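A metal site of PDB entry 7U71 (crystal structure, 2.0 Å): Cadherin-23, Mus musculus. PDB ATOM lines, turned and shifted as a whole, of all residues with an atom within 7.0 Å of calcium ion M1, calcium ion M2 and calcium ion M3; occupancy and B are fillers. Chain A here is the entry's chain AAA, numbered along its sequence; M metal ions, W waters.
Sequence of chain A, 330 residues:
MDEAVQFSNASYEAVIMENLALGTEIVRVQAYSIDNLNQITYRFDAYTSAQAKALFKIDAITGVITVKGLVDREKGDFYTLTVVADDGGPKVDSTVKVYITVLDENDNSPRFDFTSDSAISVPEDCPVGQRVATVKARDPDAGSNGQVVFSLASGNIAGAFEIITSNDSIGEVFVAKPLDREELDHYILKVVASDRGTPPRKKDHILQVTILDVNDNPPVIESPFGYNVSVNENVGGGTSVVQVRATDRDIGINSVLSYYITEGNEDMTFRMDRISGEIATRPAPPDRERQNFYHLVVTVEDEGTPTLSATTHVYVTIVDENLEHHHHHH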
ATOM      1  N   GLU A  18      -4.296   4.168 -10.864  1.00  0.00           N
ATOM      2  CA  GLU A  18      -4.445   3.610 -12.226  1.00  0.00           C
ATOM      3  C   GLU A  18      -5.258   4.597 -13.092  1.00  0.00           C
ATOM      4  O   GLU A  18      -5.993   5.428 -12.520  1.00  0.00           O
ATOM      5  CB  GLU A  18      -5.062   2.214 -12.199  1.00  0.00           C
ATOM      6  CG  GLU A  18      -6.494   2.153 -11.686  1.00  0.00           C
ATOM      7  CD  GLU A  18      -7.067   0.775 -11.894  1.00  0.00           C
ATOM      8  OE1 GLU A  18      -7.910   0.334 -11.056  1.00  0.00           O
ATOM      9  OE2 GLU A  18      -6.654   0.123 -12.923  1.00  0.00           O
ATOM     10  N   ASN A  19      -5.063   4.527 -14.412  1.00  0.00           N
ATOM     11  CA  ASN A  19      -5.829   5.294 -15.429  1.00  0.00           C
ATOM     12  C   ASN A  19      -5.428   6.784 -15.353  1.00  0.00           C
ATOM     13  O   ASN A  19      -6.129   7.622 -15.910  1.00  0.00           O
ATOM     14  CB  ASN A  19      -7.333   5.110 -15.264  1.00  0.00           C
ATOM     15  CG  ASN A  19      -7.726   3.647 -15.304  1.00  0.00           C
ATOM     16  OD1 ASN A  19      -7.207   2.880 -16.113  1.00  0.00           O
ATOM     17  ND2 ASN A  19      -8.573   3.231 -14.389  1.00  0.00           N
ATOM     18  N   VAL A  71      -1.899   2.938 -17.502  1.00  0.00           N
ATOM     19  CA  VAL A  71      -1.547   2.235 -16.235  1.00  0.00           C
ATOM     20  C   VAL A  71      -2.837   1.578 -15.687  1.00  0.00           C
ATOM     21  O   VAL A  71      -3.800   2.287 -15.360  1.00  0.00           O
ATOM     22  CB  VAL A  71      -0.904   3.208 -15.227  1.00  0.00           C
ATOM     23  CG1 VAL A  71      -0.523   2.508 -13.938  1.00  0.00           C
ATOM     24  CG2 VAL A  71       0.311   3.914 -15.849  1.00  0.00           C
ATOM     25  N   ASP A  72      -2.850   0.256 -15.691  1.00  0.00           N
ATOM     26  CA  ASP A  72      -4.010  -0.605 -15.354  1.00  0.00           C
ATOM     27  C   ASP A  72      -3.565  -1.477 -14.172  1.00  0.00           C
ATOM     28  O   ASP A  72      -2.790  -2.418 -14.396  1.00  0.00           O
ATOM     29  CB  ASP A  72      -4.394  -1.528 -16.509  1.00  0.00           C
ATOM     30  CG  ASP A  72      -5.649  -2.371 -16.252  1.00  0.00           C
ATOM     31  OD1 ASP A  72      -6.185  -2.367 -15.111  1.00  0.00           O
ATOM     32  OD2 ASP A  72      -6.053  -3.052 -17.198  1.00  0.00           O
ATOM     33  N   ARG A  73      -4.070  -1.210 -12.977  1.00  0.00           N
ATOM     34  CA  ARG A  73      -3.685  -2.007 -11.782  1.00  0.00           C
ATOM     35  C   ARG A  73      -4.027  -3.477 -12.021  1.00  0.00           C
ATOM     36  O   ARG A  73      -3.338  -4.288 -11.429  1.00  0.00           O
ATOM     37  CB  ARG A  73      -4.423  -1.541 -10.523  1.00  0.00           C
ATOM     38  CG  ARG A  73      -3.861  -2.091  -9.231  1.00  0.00           C
ATOM     39  CD  ARG A  73      -4.877  -2.129  -8.099  1.00  0.00           C
ATOM     40  NE  ARG A  73      -5.889  -3.105  -8.435  1.00  0.00           N
ATOM     41  CZ  ARG A  73      -5.821  -4.420  -8.283  1.00  0.00           C
ATOM     42  NH1 ARG A  73      -4.833  -4.981  -7.618  1.00  0.00           N
ATOM     43  NH2 ARG A  73      -6.815  -5.163  -8.732  1.00  0.00           N
ATOM     44  N   GLU A  74      -5.111  -3.780 -12.748  1.00  0.00           N
ATOM     45  CA  GLU A  74      -5.504  -5.193 -12.960  1.00  0.00           C
ATOM     46  C   GLU A  74      -4.459  -5.873 -13.848  1.00  0.00           C
ATOM     47  O   GLU A  74      -4.546  -7.118 -13.941  1.00  0.00           O
ATOM     48  CB  GLU A  74      -6.925  -5.309 -13.536  1.00  0.00           C
ATOM     49  CG  GLU A  74      -8.003  -5.047 -12.493  1.00  0.00           C
ATOM     50  CD  GLU A  74      -8.137  -3.621 -11.986  1.00  0.00           C
ATOM     51  OE1 GLU A  74      -8.352  -2.687 -12.800  1.00  0.00           O
ATOM     52  OE2 GLU A  74      -8.045  -3.450 -10.750  1.00  0.00           O
ATOM     53  N   LYS A  75      -3.524  -5.132 -14.481  1.00  0.00           N
ATOM     54  CA  LYS A  75      -2.405  -5.772 -15.250  1.00  0.00           C
ATOM     55  C   LYS A  75      -1.097  -5.757 -14.458  1.00  0.00           C
ATOM     56  O   LYS A  75      -0.156  -6.377 -14.915  1.00  0.00           O
ATOM     57  CB  LYS A  75      -2.211  -5.077 -16.608  1.00  0.00           C
ATOM     58  CG  LYS A  75      -3.277  -5.394 -17.637  1.00  0.00           C
ATOM     59  CD  LYS A  75      -2.994  -4.739 -18.983  1.00  0.00           C
ATOM     60  CE  LYS A  75      -4.238  -4.400 -19.774  1.00  0.00           C
ATOM     61  NZ  LYS A  75      -5.033  -5.603 -20.108  1.00  0.00           N
ATOM     62  N   LEU A 103      -2.296   2.343  -7.419  1.00  0.00           N
ATOM     63  CA  LEU A 103      -3.526   2.139  -6.604  1.00  0.00           C
ATOM     64  C   LEU A 103      -4.730   1.827  -7.509  1.00  0.00           C
ATOM     65  O   LEU A 103      -4.720   2.107  -8.710  1.00  0.00           O
ATOM     66  CB  LEU A 103      -3.764   3.381  -5.724  1.00  0.00           C
ATOM     67  CG  LEU A 103      -2.587   3.808  -4.862  1.00  0.00           C
ATOM     68  CD1 LEU A 103      -2.979   5.067  -4.075  1.00  0.00           C
ATOM     69  CD2 LEU A 103      -2.211   2.681  -3.913  1.00  0.00           C
ATOM     70  N   ASP A 104      -5.762   1.278  -6.896  1.00  0.00           N
ATOM     71  CA  ASP A 104      -6.983   0.749  -7.538  1.00  0.00           C
ATOM     72  C   ASP A 104      -8.023   1.843  -7.734  1.00  0.00           C
ATOM     73  O   ASP A 104      -8.320   2.539  -6.787  1.00  0.00           O
ATOM     74  CB  ASP A 104      -7.604  -0.332  -6.673  1.00  0.00           C
ATOM     75  CG  ASP A 104      -8.683  -1.111  -7.394  1.00  0.00           C
ATOM     76  OD1 ASP A 104      -8.480  -1.449  -8.563  1.00  0.00           O
ATOM     77  OD2 ASP A 104      -9.703  -1.392  -6.758  1.00  0.00           O
ATOM     78  N   GLU A 105      -8.586   1.936  -8.911  1.00  0.00           N
ATOM     79  CA  GLU A 105      -9.906   2.563  -9.190  1.00  0.00           C
ATOM     80  C   GLU A 105     -10.975   1.464  -9.262  1.00  0.00           C
ATOM     81  O   GLU A 105     -10.670   0.339  -9.712  1.00  0.00           O
ATOM     82  CB  GLU A 105      -9.903   3.295 -10.534  1.00  0.00           C
ATOM     83  CG  GLU A 105      -9.019   4.527 -10.537  1.00  0.00           C
ATOM     84  CD  GLU A 105      -9.390   5.563 -11.591  1.00  0.00           C
ATOM     85  OE1 GLU A 105      -9.781   5.175 -12.713  1.00  0.00           O
ATOM     86  OE2 GLU A 105      -9.266   6.778 -11.266  1.00  0.00           O
ATOM     87  N   ASN A 106     -12.170   1.763  -8.812  1.00  0.00           N
ATOM     88  CA  ASN A 106     -13.328   0.873  -9.028  1.00  0.00           C
ATOM     89  C   ASN A 106     -13.725   0.981 -10.495  1.00  0.00           C
ATOM     90  O   ASN A 106     -14.783   1.567 -10.802  1.00  0.00           O
ATOM     91  CB  ASN A 106     -14.489   1.184  -8.111  1.00  0.00           C
ATOM     92  CG  ASN A 106     -15.461   0.022  -8.125  1.00  0.00           C
ATOM     93  OD1 ASN A 106     -15.108  -1.097  -8.543  1.00  0.00           O
ATOM     94  ND2 ASN A 106     -16.684   0.283  -7.721  1.00  0.00           N
ATOM     95  N   ASP A 107     -12.918   0.413 -11.406  1.00  0.00           N
ATOM     96  CA  ASP A 107     -13.165   0.573 -12.853  1.00  0.00           C
ATOM     97  C   ASP A 107     -13.725  -0.712 -13.444  1.00  0.00           C
ATOM     98  O   ASP A 107     -13.886  -0.747 -14.668  1.00  0.00           O
ATOM     99  CB  ASP A 107     -11.926   1.106 -13.585  1.00  0.00           C
ATOM    100  CG  ASP A 107     -10.648   0.265 -13.484  1.00  0.00           C
ATOM    101  OD1 ASP A 107     -10.547  -0.642 -12.590  1.00  0.00           O
ATOM    102  OD2 ASP A 107      -9.729   0.571 -14.273  1.00  0.00           O
ATOM    103  N   ASN A 108     -14.111  -1.706 -12.633  1.00  0.00           N
ATOM    104  CA  ASN A 108     -14.704  -2.950 -13.171  1.00  0.00           C
ATOM    105  C   ASN A 108     -16.012  -3.236 -12.427  1.00  0.00           C
ATOM    106  O   ASN A 108     -16.116  -2.915 -11.229  1.00  0.00           O
ATOM    107  CB  ASN A 108     -13.739  -4.135 -13.096  1.00  0.00           C
ATOM    108  CG  ASN A 108     -12.543  -3.961 -14.019  1.00  0.00           C
ATOM    109  OD1 ASN A 108     -12.630  -4.335 -15.197  1.00  0.00           O
ATOM    110  ND2 ASN A 108     -11.491  -3.300 -13.562  1.00  0.00           N
ATOM    111  N   SER A 109     -17.006  -3.737 -13.174  1.00  0.00           N
ATOM    112  CA  SER A 109     -18.293  -4.204 -12.641  1.00  0.00           C
ATOM    113  C   SER A 109     -18.169  -5.707 -12.451  1.00  0.00           C
ATOM    114  O   SER A 109     -17.327  -6.317 -13.088  1.00  0.00           O
ATOM    115  CB  SER A 109     -19.480  -3.879 -13.559  1.00  0.00           C
ATOM    116  OG  SER A 109     -19.493  -2.498 -13.791  1.00  0.00           O
ATOM    117  N   PRO A 110     -18.977  -6.310 -11.551  1.00  0.00           N
ATOM    118  CA  PRO A 110     -19.055  -7.762 -11.494  1.00  0.00           C
ATOM    119  C   PRO A 110     -19.535  -8.320 -12.834  1.00  0.00           C
ATOM    120  O   PRO A 110     -20.322  -7.685 -13.512  1.00  0.00           O
ATOM    121  CB  PRO A 110     -20.061  -7.999 -10.387  1.00  0.00           C
ATOM    122  CG  PRO A 110     -20.029  -6.742  -9.504  1.00  0.00           C
ATOM    123  CD  PRO A 110     -19.741  -5.624 -10.486  1.00  0.00           C
ATOM    124  N   ASP A 139     -15.222  -9.884  -9.869  1.00  0.00           N
ATOM    125  CA  ASP A 139     -14.900  -8.449  -9.991  1.00  0.00           C
ATOM    126  C   ASP A 139     -13.402  -8.379  -9.718  1.00  0.00           C
ATOM    127  O   ASP A 139     -12.944  -8.821  -8.686  1.00  0.00           O
ATOM    128  CB  ASP A 139     -15.738  -7.613  -9.009  1.00  0.00           C
ATOM    129  CG  ASP A 139     -15.551  -6.120  -9.219  1.00  0.00           C
ATOM    130  OD1 ASP A 139     -14.386  -5.695  -9.376  1.00  0.00           O
ATOM    131  OD2 ASP A 139     -16.595  -5.389  -9.227  1.00  0.00           O
ATOM    132  N   PRO A 140     -12.592  -8.004 -10.699  1.00  0.00           N
ATOM    133  CA  PRO A 140     -11.139  -8.084 -10.533  1.00  0.00           C
ATOM    134  C   PRO A 140     -10.525  -6.855  -9.848  1.00  0.00           C
ATOM    135  O   PRO A 140      -9.309  -6.805  -9.719  1.00  0.00           O
ATOM    136  CB  PRO A 140     -10.697  -8.206 -11.994  1.00  0.00           C
ATOM    137  CG  PRO A 140     -11.677  -7.357 -12.752  1.00  0.00           C
ATOM    138  CD  PRO A 140     -13.002  -7.558 -12.045  1.00  0.00           C
ATOM    139  N   ASP A 141     -11.334  -5.907  -9.363  1.00  0.00           N
ATOM    140  CA  ASP A 141     -10.765  -4.772  -8.592  1.00  0.00           C
ATOM    141  C   ASP A 141     -10.237  -5.278  -7.229  1.00  0.00           C
ATOM    142  O   ASP A 141     -10.490  -6.444  -6.847  1.00  0.00           O
ATOM    143  CB  ASP A 141     -11.761  -3.626  -8.489  1.00  0.00           C
ATOM    144  CG  ASP A 141     -12.141  -3.035  -9.819  1.00  0.00           C
ATOM    145  OD1 ASP A 141     -11.230  -2.848 -10.648  1.00  0.00           O
ATOM    146  OD2 ASP A 141     -13.367  -2.820 -10.058  1.00  0.00           O
ATOM    147  N   ALA A 142      -9.611  -4.417  -6.446  1.00  0.00           N
ATOM    148  CA  ALA A 142      -8.946  -4.768  -5.164  1.00  0.00           C
ATOM    149  C   ALA A 142      -9.899  -4.438  -4.014  1.00  0.00           C
ATOM    150  O   ALA A 142     -10.733  -3.502  -4.159  1.00  0.00           O
ATOM    151  CB  ALA A 142      -7.603  -4.031  -5.042  1.00  0.00           C
ATOM    152  N   SER A 144     -12.642  -3.882  -1.304  1.00  0.00           N
ATOM    153  CA  SER A 144     -14.107  -3.624  -1.391  1.00  0.00           C
ATOM    154  C   SER A 144     -14.573  -3.524  -2.859  1.00  0.00           C
ATOM    155  O   SER A 144     -15.681  -3.969  -3.195  1.00  0.00           O
ATOM    156  CB  SER A 144     -14.433  -2.313  -0.701  1.00  0.00           C
ATOM    157  OG  SER A 144     -14.333  -2.427   0.700  1.00  0.00           O
ATOM    158  N   ASN A 145     -13.799  -2.814  -3.679  1.00  0.00           N
ATOM    159  CA  ASN A 145     -14.075  -2.584  -5.131  1.00  0.00           C
ATOM    160  C   ASN A 145     -14.237  -3.911  -5.855  1.00  0.00           C
ATOM    161  O   ASN A 145     -14.868  -3.908  -6.918  1.00  0.00           O
ATOM    162  CB  ASN A 145     -12.985  -1.779  -5.839  1.00  0.00           C
ATOM    163  CG  ASN A 145     -12.842  -0.380  -5.282  1.00  0.00           C
ATOM    164  OD1 ASN A 145     -13.791   0.172  -4.702  1.00  0.00           O
ATOM    165  ND2 ASN A 145     -11.663   0.213  -5.468  1.00  0.00           N
ATOM    166  N   GLY A 146     -13.678  -4.991  -5.302  1.00  0.00           N
ATOM    167  CA  GLY A 146     -13.738  -6.329  -5.906  1.00  0.00           C
ATOM    168  C   GLY A 146     -14.582  -7.334  -5.148  1.00  0.00           C
ATOM    169  O   GLY A 146     -14.687  -8.476  -5.628  1.00  0.00           O
ATOM    170  N   GLN A 147     -15.115  -6.991  -3.988  1.00  0.00           N
ATOM    171  CA  GLN A 147     -15.988  -7.936  -3.243  1.00  0.00           C
ATOM    172  C   GLN A 147     -17.397  -7.934  -3.839  1.00  0.00           C
ATOM    173  O   GLN A 147     -17.895  -6.843  -4.045  1.00  0.00           O
ATOM    174  CB  GLN A 147     -16.145  -7.448  -1.803  1.00  0.00           C
ATOM    175  CG  GLN A 147     -14.934  -7.726  -0.953  1.00  0.00           C
ATOM    176  CD  GLN A 147     -15.155  -7.118   0.410  1.00  0.00           C
ATOM    177  OE1 GLN A 147     -15.765  -6.070   0.573  1.00  0.00           O
ATOM    178  NE2 GLN A 147     -14.720  -7.837   1.430  1.00  0.00           N
ATOM    179  N   ASP A 195     -20.683  -4.856  -6.464  1.00  0.00           N
ATOM    180  CA  ASP A 195     -19.413  -4.774  -5.697  1.00  0.00           C
ATOM    181  C   ASP A 195     -19.656  -3.931  -4.438  1.00  0.00           C
ATOM    182  O   ASP A 195     -20.799  -3.515  -4.180  1.00  0.00           O
ATOM    183  CB  ASP A 195     -18.219  -4.343  -6.554  1.00  0.00           C
ATOM    184  CG  ASP A 195     -18.215  -2.912  -7.070  1.00  0.00           C
ATOM    185  OD1 ASP A 195     -18.864  -2.017  -6.413  1.00  0.00           O
ATOM    186  OD2 ASP A 195     -17.561  -2.703  -8.141  1.00  0.00           O
ATOM    187  N   ARG A 196     -18.629  -3.723  -3.626  1.00  0.00           N
ATOM    188  CA  ARG A 196     -18.749  -2.891  -2.410  1.00  0.00           C
ATOM    189  C   ARG A 196     -17.943  -1.615  -2.629  1.00  0.00           C
ATOM    190  O   ARG A 196     -17.461  -1.033  -1.660  1.00  0.00           O
ATOM    191  CB  ARG A 196     -18.325  -3.716  -1.198  1.00  0.00           C
ATOM    192  CG  ARG A 196     -19.287  -4.859  -0.879  1.00  0.00           C
ATOM    193  CD  ARG A 196     -19.264  -5.264   0.590  1.00  0.00           C
ATOM    194  NE  ARG A 196     -19.914  -6.550   0.881  1.00  0.00           N
ATOM    195  CZ  ARG A 196     -21.170  -6.738   1.273  1.00  0.00           C
ATOM    196  NH1 ARG A 196     -21.990  -5.727   1.431  1.00  0.00           N
ATOM    197  NH2 ARG A 196     -21.599  -7.971   1.546  1.00  0.00           N
ATOM    198  N   GLY A 197     -17.838  -1.192  -3.871  1.00  0.00           N
ATOM    199  CA  GLY A 197     -17.289   0.130  -4.143  1.00  0.00           C
ATOM    200  C   GLY A 197     -18.175   1.186  -3.519  1.00  0.00           C
ATOM    201  O   GLY A 197     -19.355   0.916  -3.239  1.00  0.00           O
ATOM    202  N   ARG A 201     -20.698  -0.641  -8.108  1.00  0.00           N
ATOM    203  CA  ARG A 201     -21.013  -1.009  -9.504  1.00  0.00           C
ATOM    204  C   ARG A 201     -21.817  -2.304  -9.505  1.00  0.00           C
ATOM    205  O   ARG A 201     -21.510  -3.217  -8.732  1.00  0.00           O
ATOM    206  CB  ARG A 201     -19.689  -1.068 -10.245  1.00  0.00           C
ATOM    207  CG  ARG A 201     -19.099   0.312 -10.525  1.00  0.00           C
ATOM    208  CD  ARG A 201     -17.751   0.176 -11.180  1.00  0.00           C
ATOM    209  NE  ARG A 201     -17.907  -0.212 -12.553  1.00  0.00           N
ATOM    210  CZ  ARG A 201     -17.361   0.391 -13.600  1.00  0.00           C
ATOM    211  NH1 ARG A 201     -16.556   1.433 -13.481  1.00  0.00           N
ATOM    212  NH2 ARG A 201     -17.648  -0.064 -14.795  1.00  0.00           N
HETATM  213 CA    CA M   1      -9.329  -1.393 -10.707  1.00  0.00          CA
HETATM  214 CA    CA M   2      -8.026  -1.078 -14.378  1.00  0.00          CA
HETATM  215 CA    CA M   3     -15.483  -3.419  -9.057  1.00  0.00          CA
HETATM  216  O   HOH W   1      -9.467  -2.629 -15.752  1.00  0.00           O
HETATM  217  O   HOH W   2      -7.357   0.197 -16.243  1.00  0.00           O
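ND2 of Asn 108 lies close to OE1 of Glu 74. NH2 of Arg 73 lies close to OE2 of Glu 74, 2.9 Å away. NE of Arg 73 lies close to OD1 of Asp 104, at 3.1 Å. The side-chain carboxylate of Asp 104 lies within hydrogen-bond range of the backbone NH of Ala 142. The side-chain carboxylate (OD2) of Asp 107 sits close to the side-chain amide nitrogen (ND2) of Asn 19, at 2.9 Å. The backbone NH of Arg 201 sits at hydrogen-bond distance from the side-chain carboxylate of Asp 195, 2.9 Å away. The backbone NH of Gly 197 sits at hydrogen-bond distance from the side-chain carboxylate of Asp 195 (2.9 Å). OE1 of Glu 105 is in hydrogen-bond range of ND2 of Asn 19 (2.8 Å).
Six residues have an atom within 4 Å of calcium ion M1: Glu 18, Glu 74, Asp 104, Glu 105, Asp 107 and Asp 141. The nearest printed residue that does not touch calcium ion M1 is Asn 108 (4.1 Å).
Four residues have an atom within 4 Å of calcium ion M2: Glu 18, Asp 72, Glu 74 and Asp 107.
Six residues have an atom within 4 Å of calcium ion M3: Asn 106, Asn 108, Asp 139, Asp 141, Asn 145 and Asp 195.
Calcium ion M1 is bound by OE1 of Glu 18, OD1 of Asp 104, OD1 of Asp 107, OD1 of Asp 141, O of Glu 105, OE2 of Glu 74 and OE1 of Glu 74.
Calcium ion M2 is bound by the side-chain carboxylate of Glu 74, the side-chain carboxylate of Glu 18, water W2, the side-chain carboxylate of Asp 72, the side-chain carboxylate of Asp 107 and water W1. Calcium ion M2 has six donor atoms within binding distance. Slightly farther from calcium ion M2 lies OD1 of Asp 107 (3.1 Å).
Calcium ion M3 is bound by the side-chain carboxylate (OD2) of Asp 139 (2.3 Å), the backbone carbonyl oxygen (O) of Asn 145 (2.3 Å), the backbone carbonyl oxygen (O) of Asn 108 (2.3 Å), the side-chain carboxylate (OD2) of Asp 195 (2.4 Å), the side-chain amide oxygen (OD1) of Asn 106 (2.4 Å), the side-chain carboxylate (OD2) of Asp 141 (2.4 Å) and the side-chain carboxylate (OD1) of Asp 139 (2.5 Å). Calcium ion M3 has seven donor atoms within binding distance.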
